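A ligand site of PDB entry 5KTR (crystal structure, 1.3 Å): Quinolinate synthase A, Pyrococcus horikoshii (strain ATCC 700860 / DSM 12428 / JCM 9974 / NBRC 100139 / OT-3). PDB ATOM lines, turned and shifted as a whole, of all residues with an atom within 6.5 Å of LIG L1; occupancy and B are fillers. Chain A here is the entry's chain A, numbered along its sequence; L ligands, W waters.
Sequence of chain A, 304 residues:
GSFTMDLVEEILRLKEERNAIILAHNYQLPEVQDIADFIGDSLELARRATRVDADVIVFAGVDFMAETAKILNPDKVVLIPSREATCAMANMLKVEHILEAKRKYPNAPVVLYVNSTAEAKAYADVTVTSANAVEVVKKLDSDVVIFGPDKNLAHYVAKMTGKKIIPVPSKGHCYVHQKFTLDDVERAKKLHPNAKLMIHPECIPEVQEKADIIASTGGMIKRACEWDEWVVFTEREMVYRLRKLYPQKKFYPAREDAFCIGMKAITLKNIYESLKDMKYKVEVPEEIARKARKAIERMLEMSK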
ATOM      1  N   HIS A  25     -28.432  23.435  38.366  1.00  0.00           N
ATOM      2  CA  HIS A  25     -28.175  22.581  37.228  1.00  0.00           C
ATOM      3  C   HIS A  25     -28.791  21.191  37.448  1.00  0.00           C
ATOM      4  O   HIS A  25     -28.976  20.722  38.587  1.00  0.00           O
ATOM      5  CB  HIS A  25     -26.670  22.441  36.966  1.00  0.00           C
ATOM      6  CG  HIS A  25     -26.378  21.729  35.695  1.00  0.00           C
ATOM      7  ND1 HIS A  25     -26.092  20.384  35.647  1.00  0.00           N
ATOM      8  CD2 HIS A  25     -26.387  22.167  34.407  1.00  0.00           C
ATOM      9  CE1 HIS A  25     -25.911  20.024  34.385  1.00  0.00           C
ATOM     10  NE2 HIS A  25     -26.104  21.086  33.615  1.00  0.00           N
ATOM     11  N   ASN A  26     -29.078  20.521  36.326  1.00  0.00           N
ATOM     12  CA  ASN A  26     -29.648  19.173  36.315  1.00  0.00           C
ATOM     13  C   ASN A  26     -28.801  18.116  37.027  1.00  0.00           C
ATOM     14  O   ASN A  26     -29.330  17.050  37.354  1.00  0.00           O
ATOM     15  CB  ASN A  26     -29.902  18.730  34.868  1.00  0.00           C
ATOM     16  CG  ASN A  26     -31.094  19.427  34.255  1.00  0.00           C
ATOM     17  OD1 ASN A  26     -32.095  19.652  34.925  1.00  0.00           O
ATOM     18  ND2 ASN A  26     -30.993  19.770  32.964  1.00  0.00           N
ATOM     19  N   TYR A  27     -27.507  18.365  37.278  1.00  0.00           N
ATOM     20  CA  TYR A  27     -26.664  17.390  37.972  1.00  0.00           C
ATOM     21  C   TYR A  27     -26.612  17.604  39.471  1.00  0.00           C
ATOM     22  O   TYR A  27     -25.844  16.919  40.156  1.00  0.00           O
ATOM     23  CB  TYR A  27     -25.210  17.427  37.450  1.00  0.00           C
ATOM     24  CG  TYR A  27     -25.015  17.133  35.974  1.00  0.00           C
ATOM     25  CD1 TYR A  27     -25.966  16.444  35.233  1.00  0.00           C
ATOM     26  CD2 TYR A  27     -23.869  17.557  35.311  1.00  0.00           C
ATOM     27  CE1 TYR A  27     -25.785  16.193  33.875  1.00  0.00           C
ATOM     28  CE2 TYR A  27     -23.680  17.326  33.946  1.00  0.00           C
ATOM     29  CZ  TYR A  27     -24.631  16.638  33.235  1.00  0.00           C
ATOM     30  OH  TYR A  27     -24.437  16.405  31.887  1.00  0.00           O
ATOM     31  N   GLY A  40     -32.120  23.604  35.146  1.00  0.00           N
ATOM     32  CA  GLY A  40     -31.967  23.468  33.712  1.00  0.00           C
ATOM     33  C   GLY A  40     -30.550  23.115  33.306  1.00  0.00           C
ATOM     34  O   GLY A  40     -29.682  22.882  34.148  1.00  0.00           O
ATOM     35  N   ASP A  41     -30.337  23.067  31.974  1.00  0.00           N
ATOM     36  CA  ASP A  41     -29.020  22.854  31.380  1.00  0.00           C
ATOM     37  C   ASP A  41     -28.307  24.190  31.246  1.00  0.00           C
ATOM     38  O   ASP A  41     -28.798  25.240  31.702  1.00  0.00           O
ATOM     39  CB  ASP A  41     -29.121  22.057  30.067  1.00  0.00           C
ATOM     40  CG  ASP A  41     -29.656  22.881  28.883  1.00  0.00           C
ATOM     41  OD1 ASP A  41     -30.068  24.051  29.080  1.00  0.00           O
ATOM     42  OD2 ASP A  41     -29.654  22.345  27.736  1.00  0.00           O
ATOM     43  N   SER A  42     -27.123  24.188  30.625  1.00  0.00           N
ATOM     44  CA  SER A  42     -26.316  25.406  30.623  1.00  0.00           C
ATOM     45  C   SER A  42     -26.978  26.528  29.819  1.00  0.00           C
ATOM     46  O   SER A  42     -26.950  27.686  30.238  1.00  0.00           O
ATOM     47  CB  SER A  42     -24.906  25.118  30.109  1.00  0.00           C
ATOM     48  OG  SER A  42     -24.202  24.309  31.042  1.00  0.00           O
ATOM     49  N   LEU A  43     -27.589  26.194  28.675  1.00  0.00           N
ATOM     50  CA  LEU A  43     -28.254  27.222  27.874  1.00  0.00           C
ATOM     51  C   LEU A  43     -29.477  27.771  28.592  1.00  0.00           C
ATOM     52  O   LEU A  43     -29.705  28.991  28.607  1.00  0.00           O
ATOM     53  CB  LEU A  43     -28.637  26.661  26.507  1.00  0.00           C
ATOM     54  CG  LEU A  43     -29.410  27.643  25.611  1.00  0.00           C
ATOM     55  CD1 LEU A  43     -28.640  28.940  25.390  1.00  0.00           C
ATOM     56  CD2 LEU A  43     -29.706  26.971  24.289  1.00  0.00           C
ATOM     57  N   PHE A  64     -18.155  28.337  36.766  1.00  0.00           N
ATOM     58  CA  PHE A  64     -18.313  28.954  35.440  1.00  0.00           C
ATOM     59  C   PHE A  64     -19.773  29.328  35.184  1.00  0.00           C
ATOM     60  O   PHE A  64     -20.053  30.373  34.596  1.00  0.00           O
ATOM     61  CB  PHE A  64     -17.662  28.126  34.306  1.00  0.00           C
ATOM     62  CG  PHE A  64     -18.470  26.912  33.807  1.00  0.00           C
ATOM     63  CD1 PHE A  64     -19.608  27.065  33.036  1.00  0.00           C
ATOM     64  CD2 PHE A  64     -18.017  25.616  34.041  1.00  0.00           C
ATOM     65  CE1 PHE A  64     -20.311  25.963  32.570  1.00  0.00           C
ATOM     66  CE2 PHE A  64     -18.706  24.518  33.572  1.00  0.00           C
ATOM     67  CZ  PHE A  64     -19.865  24.699  32.843  1.00  0.00           C
ATOM     68  N   MET A  65     -20.701  28.504  35.671  1.00  0.00           N
ATOM     69  CA  MET A  65     -22.113  28.800  35.495  1.00  0.00           C
ATOM     70  C   MET A  65     -22.521  30.011  36.324  1.00  0.00           C
ATOM     71  O   MET A  65     -23.258  30.874  35.849  1.00  0.00           O
ATOM     72  CB  MET A  65     -22.955  27.607  35.912  1.00  0.00           C
ATOM     73  CG  MET A  65     -22.748  26.392  35.056  1.00  0.00           C
ATOM     74  SD  MET A  65     -23.675  24.977  35.681  1.00  0.00           S
ATOM     75  CE  MET A  65     -23.217  23.809  34.387  1.00  0.00           C
ATOM     76  N   TYR A 113     -17.386  26.982  24.331  1.00  0.00           N
ATOM     77  CA  TYR A 113     -18.319  26.298  25.178  1.00  0.00           C
ATOM     78  C   TYR A 113     -18.432  27.086  26.467  1.00  0.00           C
ATOM     79  O   TYR A 113     -17.447  27.643  26.948  1.00  0.00           O
ATOM     80  CB  TYR A 113     -17.732  24.914  25.463  1.00  0.00           C
ATOM     81  CG  TYR A 113     -18.701  23.828  25.852  1.00  0.00           C
ATOM     82  CD1 TYR A 113     -18.231  22.620  26.354  1.00  0.00           C
ATOM     83  CD2 TYR A 113     -20.073  23.976  25.700  1.00  0.00           C
ATOM     84  CE1 TYR A 113     -19.083  21.619  26.701  1.00  0.00           C
ATOM     85  CE2 TYR A 113     -20.934  22.963  26.060  1.00  0.00           C
ATOM     86  CZ  TYR A 113     -20.435  21.790  26.568  1.00  0.00           C
ATOM     87  OH  TYR A 113     -21.291  20.791  26.927  1.00  0.00           O
ATOM     88  N   VAL A 114     -19.656  27.170  26.989  1.00  0.00           N
ATOM     89  CA  VAL A 114     -19.871  27.883  28.235  1.00  0.00           C
ATOM     90  C   VAL A 114     -19.057  27.276  29.359  1.00  0.00           C
ATOM     91  O   VAL A 114     -18.706  27.976  30.312  1.00  0.00           O
ATOM     92  CB  VAL A 114     -21.391  27.984  28.511  1.00  0.00           C
ATOM     93  CG1 VAL A 114     -21.674  28.498  29.907  1.00  0.00           C
ATOM     94  CG2 VAL A 114     -22.046  28.902  27.469  1.00  0.00           C
ATOM     95  N   ASN A 115     -18.684  25.993  29.244  1.00  0.00           N
ATOM     96  CA  ASN A 115     -17.736  25.382  30.167  1.00  0.00           C
ATOM     97  C   ASN A 115     -16.364  25.981  29.890  1.00  0.00           C
ATOM     98  O   ASN A 115     -15.494  25.375  29.271  1.00  0.00           O
ATOM     99  CB  ASN A 115     -17.689  23.864  29.992  1.00  0.00           C
ATOM    100  CG  ASN A 115     -19.053  23.208  30.043  1.00  0.00           C
ATOM    101  OD1 ASN A 115     -20.014  23.705  29.470  1.00  0.00           O
ATOM    102  ND2 ASN A 115     -19.132  22.071  30.724  1.00  0.00           N
ATOM    103  N   VAL A 128     -21.270  28.900  23.165  1.00  0.00           N
ATOM    104  CA  VAL A 128     -22.191  27.823  22.821  1.00  0.00           C
ATOM    105  C   VAL A 128     -22.350  26.908  24.022  1.00  0.00           C
ATOM    106  O   VAL A 128     -21.556  26.925  24.966  1.00  0.00           O
ATOM    107  CB  VAL A 128     -21.744  26.975  21.600  1.00  0.00           C
ATOM    108  CG1 VAL A 128     -21.758  27.803  20.332  1.00  0.00           C
ATOM    109  CG2 VAL A 128     -20.375  26.325  21.848  1.00  0.00           C
ATOM    110  N   THR A 129     -23.385  26.088  23.970  1.00  0.00           N
ATOM    111  CA  THR A 129     -23.564  24.975  24.891  1.00  0.00           C
ATOM    112  C   THR A 129     -23.790  23.730  24.047  1.00  0.00           C
ATOM    113  O   THR A 129     -23.858  23.782  22.821  1.00  0.00           O
ATOM    114  CB  THR A 129     -24.758  25.206  25.830  1.00  0.00           C
ATOM    115  OG1 THR A 129     -25.974  24.985  25.120  1.00  0.00           O
ATOM    116  CG2 THR A 129     -24.739  26.604  26.430  1.00  0.00           C
ATOM    117  N   SER A 130     -23.945  22.591  24.723  1.00  0.00           N
ATOM    118  CA  SER A 130     -24.233  21.365  23.991  1.00  0.00           C
ATOM    119  C   SER A 130     -25.563  21.423  23.252  1.00  0.00           C
ATOM    120  O   SER A 130     -25.755  20.694  22.269  1.00  0.00           O
ATOM    121  CB  SER A 130     -24.201  20.166  24.938  1.00  0.00           C
ATOM    122  OG  SER A 130     -22.857  19.780  25.229  1.00  0.00           O
ATOM    123  N   ALA A 131     -26.494  22.276  23.684  1.00  0.00           N
ATOM    124  CA  ALA A 131     -27.802  22.367  23.047  1.00  0.00           C
ATOM    125  C   ALA A 131     -27.780  23.142  21.738  1.00  0.00           C
ATOM    126  O   ALA A 131     -28.614  22.866  20.862  1.00  0.00           O
ATOM    127  CB  ALA A 131     -28.802  23.022  24.000  1.00  0.00           C
ATOM    128  N   LEU A 153     -17.538  17.170  22.094  1.00  0.00           N
ATOM    129  CA  LEU A 153     -18.530  18.055  21.493  1.00  0.00           C
ATOM    130  C   LEU A 153     -18.019  18.594  20.162  1.00  0.00           C
ATOM    131  O   LEU A 153     -18.793  18.704  19.194  1.00  0.00           O
ATOM    132  CB  LEU A 153     -18.864  19.198  22.456  1.00  0.00           C
ATOM    133  CG  LEU A 153     -19.866  20.241  21.931  1.00  0.00           C
ATOM    134  CD1 LEU A 153     -21.174  19.596  21.480  1.00  0.00           C
ATOM    135  CD2 LEU A 153     -20.122  21.320  22.960  1.00  0.00           C
ATOM    136  N   HIS A 177     -18.070  12.160  31.519  1.00  0.00           N
ATOM    137  CA  HIS A 177     -18.606  11.570  30.297  1.00  0.00           C
ATOM    138  C   HIS A 177     -17.622  10.654  29.604  1.00  0.00           C
ATOM    139  O   HIS A 177     -18.063   9.747  28.884  1.00  0.00           O
ATOM    140  CB  HIS A 177     -19.112  12.670  29.363  1.00  0.00           C
ATOM    141  CG  HIS A 177     -20.344  13.349  29.880  1.00  0.00           C
ATOM    142  ND1 HIS A 177     -20.284  14.463  30.694  1.00  0.00           N
ATOM    143  CD2 HIS A 177     -21.649  13.018  29.771  1.00  0.00           C
ATOM    144  CE1 HIS A 177     -21.524  14.804  31.037  1.00  0.00           C
ATOM    145  NE2 HIS A 177     -22.361  13.949  30.486  1.00  0.00           N
ATOM    146  N   HIS A 200     -25.067  12.149  25.878  1.00  0.00           N
ATOM    147  CA  HIS A 200     -24.560  13.506  25.887  1.00  0.00           C
ATOM    148  C   HIS A 200     -23.417  13.632  24.865  1.00  0.00           C
ATOM    149  O   HIS A 200     -22.620  12.704  24.726  1.00  0.00           O
ATOM    150  CB  HIS A 200     -24.034  13.839  27.273  1.00  0.00           C
ATOM    151  CG  HIS A 200     -23.928  15.309  27.532  1.00  0.00           C
ATOM    152  ND1 HIS A 200     -22.903  16.086  27.048  1.00  0.00           N
ATOM    153  CD2 HIS A 200     -24.763  16.149  28.189  1.00  0.00           C
ATOM    154  CE1 HIS A 200     -23.100  17.347  27.403  1.00  0.00           C
ATOM    155  NE2 HIS A 200     -24.222  17.407  28.101  1.00  0.00           N
ATOM    156  N   PRO A 201     -23.313  14.747  24.135  1.00  0.00           N
ATOM    157  CA  PRO A 201     -22.221  14.887  23.168  1.00  0.00           C
ATOM    158  C   PRO A 201     -20.842  15.040  23.786  1.00  0.00           C
ATOM    159  O   PRO A 201     -19.854  15.066  23.037  1.00  0.00           O
ATOM    160  CB  PRO A 201     -22.616  16.128  22.356  1.00  0.00           C
ATOM    161  CG  PRO A 201     -23.489  16.916  23.271  1.00  0.00           C
ATOM    162  CD  PRO A 201     -24.262  15.888  24.073  1.00  0.00           C
ATOM    163  N   GLU A 202     -20.732  15.139  25.117  1.00  0.00           N
ATOM    164  CA  GLU A 202     -19.420  15.062  25.753  1.00  0.00           C
ATOM    165  C   GLU A 202     -18.908  13.629  25.858  1.00  0.00           C
ATOM    166  O   GLU A 202     -17.761  13.430  26.267  1.00  0.00           O
ATOM    167  CB  GLU A 202     -19.452  15.735  27.123  1.00  0.00           C
ATOM    168  CG  GLU A 202     -19.558  17.256  27.057  1.00  0.00           C
ATOM    169  CD  GLU A 202     -19.726  17.900  28.418  1.00  0.00           C
ATOM    170  OE1 GLU A 202     -19.357  17.271  29.421  1.00  0.00           O
ATOM    171  OE2 GLU A 202     -20.225  19.040  28.504  1.00  0.00           O
ATOM    172  N   ALA A 215     -27.942  14.754  22.833  1.00  0.00           N
ATOM    173  CA  ALA A 215     -28.534  15.978  23.352  1.00  0.00           C
ATOM    174  C   ALA A 215     -27.841  16.403  24.628  1.00  0.00           C
ATOM    175  O   ALA A 215     -27.298  15.575  25.369  1.00  0.00           O
ATOM    176  CB  ALA A 215     -30.027  15.757  23.654  1.00  0.00           C
ATOM    177  N   SER A 216     -27.900  17.713  24.891  1.00  0.00           N
ATOM    178  CA  SER A 216     -27.643  18.220  26.234  1.00  0.00           C
ATOM    179  C   SER A 216     -28.708  17.691  27.182  1.00  0.00           C
ATOM    180  O   SER A 216     -29.714  17.097  26.758  1.00  0.00           O
ATOM    181  CB  SER A 216     -27.688  19.749  26.242  1.00  0.00           C
ATOM    182  OG  SER A 216     -29.041  20.201  26.213  1.00  0.00           O
ATOM    183  N   THR A 217     -28.506  17.926  28.483  1.00  0.00           N
ATOM    184  CA  THR A 217     -29.540  17.491  29.416  1.00  0.00           C
ATOM    185  C   THR A 217     -30.867  18.195  29.124  1.00  0.00           C
ATOM    186  O   THR A 217     -31.933  17.607  29.305  1.00  0.00           O
ATOM    187  CB  THR A 217     -29.122  17.729  30.871  1.00  0.00           C
ATOM    188  OG1 THR A 217     -28.944  19.136  31.103  1.00  0.00           O
ATOM    189  CG2 THR A 217     -27.851  16.969  31.240  1.00  0.00           C
ATOM    190  N   GLY A 218     -30.816  19.446  28.647  1.00  0.00           N
ATOM    191  CA  GLY A 218     -32.046  20.115  28.281  1.00  0.00           C
ATOM    192  C   GLY A 218     -32.739  19.451  27.101  1.00  0.00           C
ATOM    193  O   GLY A 218     -33.957  19.281  27.102  1.00  0.00           O
ATOM    194  N   THR A 234     -25.349  10.250  30.866  1.00  0.00           N
ATOM    195  CA  THR A 234     -24.790  11.487  31.392  1.00  0.00           C
ATOM    196  C   THR A 234     -24.635  11.314  32.907  1.00  0.00           C
ATOM    197  O   THR A 234     -24.826  10.212  33.444  1.00  0.00           O
ATOM    198  CB  THR A 234     -25.616  12.705  30.957  1.00  0.00           C
ATOM    199  OG1 THR A 234     -24.907  13.905  31.277  1.00  0.00           O
ATOM    200  CG2 THR A 234     -26.987  12.751  31.604  1.00  0.00           C
HETATM  201  C1  LIG L   1     -24.557  22.049  28.584  1.00  0.00           C
HETATM  202  O1  LIG L   1     -25.767  22.193  28.635  1.00  0.00           O
HETATM  203  O2  LIG L   1     -23.866  22.560  27.563  1.00  0.00           O
HETATM  204  C2  LIG L   1     -23.792  21.328  29.619  1.00  0.00           C
HETATM  205  C3  LIG L   1     -24.331  20.308  30.308  1.00  0.00           C
HETATM  206  C4  LIG L   1     -25.716  19.843  30.118  1.00  0.00           C
HETATM  207  O3  LIG L   1     -26.583  20.220  31.053  1.00  0.00           O
HETATM  208  O4  LIG L   1     -26.072  19.151  29.185  1.00  0.00           O
HETATM  209 FE1  LG2 L   2     -17.467  20.002  34.024  1.00  0.00          FE
HETATM  210 FE2  LG2 L   2     -18.642  18.363  35.834  1.00  0.00          FE
HETATM  211 FE3  LG2 L   2     -18.013  17.455  33.323  1.00  0.00          FE
HETATM  212 FE4  LG2 L   2     -19.957  19.333  33.638  1.00  0.00          FE
HETATM  213  S1  LG2 L   2     -19.968  17.161  34.412  1.00  0.00           S
HETATM  214  S2  LG2 L   2     -18.305  19.288  32.025  1.00  0.00           S
HETATM  215  S3  LG2 L   2     -19.131  20.538  35.431  1.00  0.00           S
HETATM  216  S4  LG2 L   2     -16.517  18.138  34.921  1.00  0.00           S
HETATM  217  O   HOH W   1     -22.250  24.723  28.606  1.00  0.00           O
HETATM  218  O   HOH W   2     -27.198  23.655  27.118  1.00  0.00           O
HETATM  219  O   HOH W   3     -21.834  18.141  31.122  1.00  0.00           O
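An oxygen (O3) of LIG L1 lies within hydrogen-bond range of a ring nitrogen (NE2) of His 25. The backbone NH (N) of Thr 217 sits at hydrogen-bond distance from an oxygen (O4) of LIG L1, at 2.8 Å. O2 of LIG L1 is in hydrogen-bond range of N of Ser 130 (2.8 Å). N of Ser 42 is in hydrogen-bond range of O1 of LIG L1 (3.1 Å). OH of Tyr 113 lies within hydrogen-bond range of O2 of LIG L1, at 3.2 Å. ND2 of Asn 115 sits close to S2 of LG2 L2, at 3.2 Å. The side-chain hydroxyl of Thr 217 is in hydrogen-bond range of an oxygen (O3) of LIG L1 (2.6 Å). An oxygen (O4) of LIG L1 lies within hydrogen-bond range of a ring nitrogen (NE2) of His 200 (2.8 Å).
Water W2 lies within hydrogen-bond range of an oxygen (O1) of LIG L1 (2.5 Å), the side-chain hydroxyl of Thr 129 (2.7 Å), the side-chain carboxylate of Asp 41 (2.9 Å) and the backbone NH of Leu 43 (3.0 Å). Water W1 lies within hydrogen-bond range of OD1 of Asn 115 (2.6 Å), O2 of LIG L1 (2.9 Å) and OG of Ser 42 (3.1 Å). Water W3 lies within hydrogen-bond range of the side-chain carboxylate (OE1) of Glu 202 (3.1 Å) and the side-chain hydroxyl (OH) of Tyr 27 (3.2 Å).
Asp 41 touches LIG L1. Thr 129 touches LIG L1 (CB to O2, 3.3 Å). Ser 216 touches LIG L1 (CB to O4, 3.4 Å). Of the 26 residues printed, 9 come within 4 Å of LIG L1. The nearest printed residue that does not touch LIG L1 is Tyr 27 (4.1 Å).
The backbone NH (N) of Tyr 27 is in hydrogen-bond range of a ring nitrogen (ND1) of His 25, 3.0 Å away. OH of Tyr 113 lies within hydrogen-bond range of OG of Ser 130. The backbone NH (N) of Gly 218 is in hydrogen-bond range of the side-chain carboxylate (OD2) of Asp 41, 3.3 Å away. The side-chain hydroxyl (OG) of Ser 216 is in hydrogen-bond range of the backbone NH (N) of Gly 218 (3.1 Å). The side-chain hydroxyl of Thr 129 sits close to the backbone NH of Ala 131 (3.1 Å). ND2 of Asn 26 sits at hydrogen-bond distance from OG1 of Thr 217 (2.8 Å). OD2 of Asp 41 sits at hydrogen-bond distance from OG of Ser 216, at 2.7 Å. ND1 of His 200 lies within hydrogen-bond range of N of Glu 202, at 3.1 Å.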
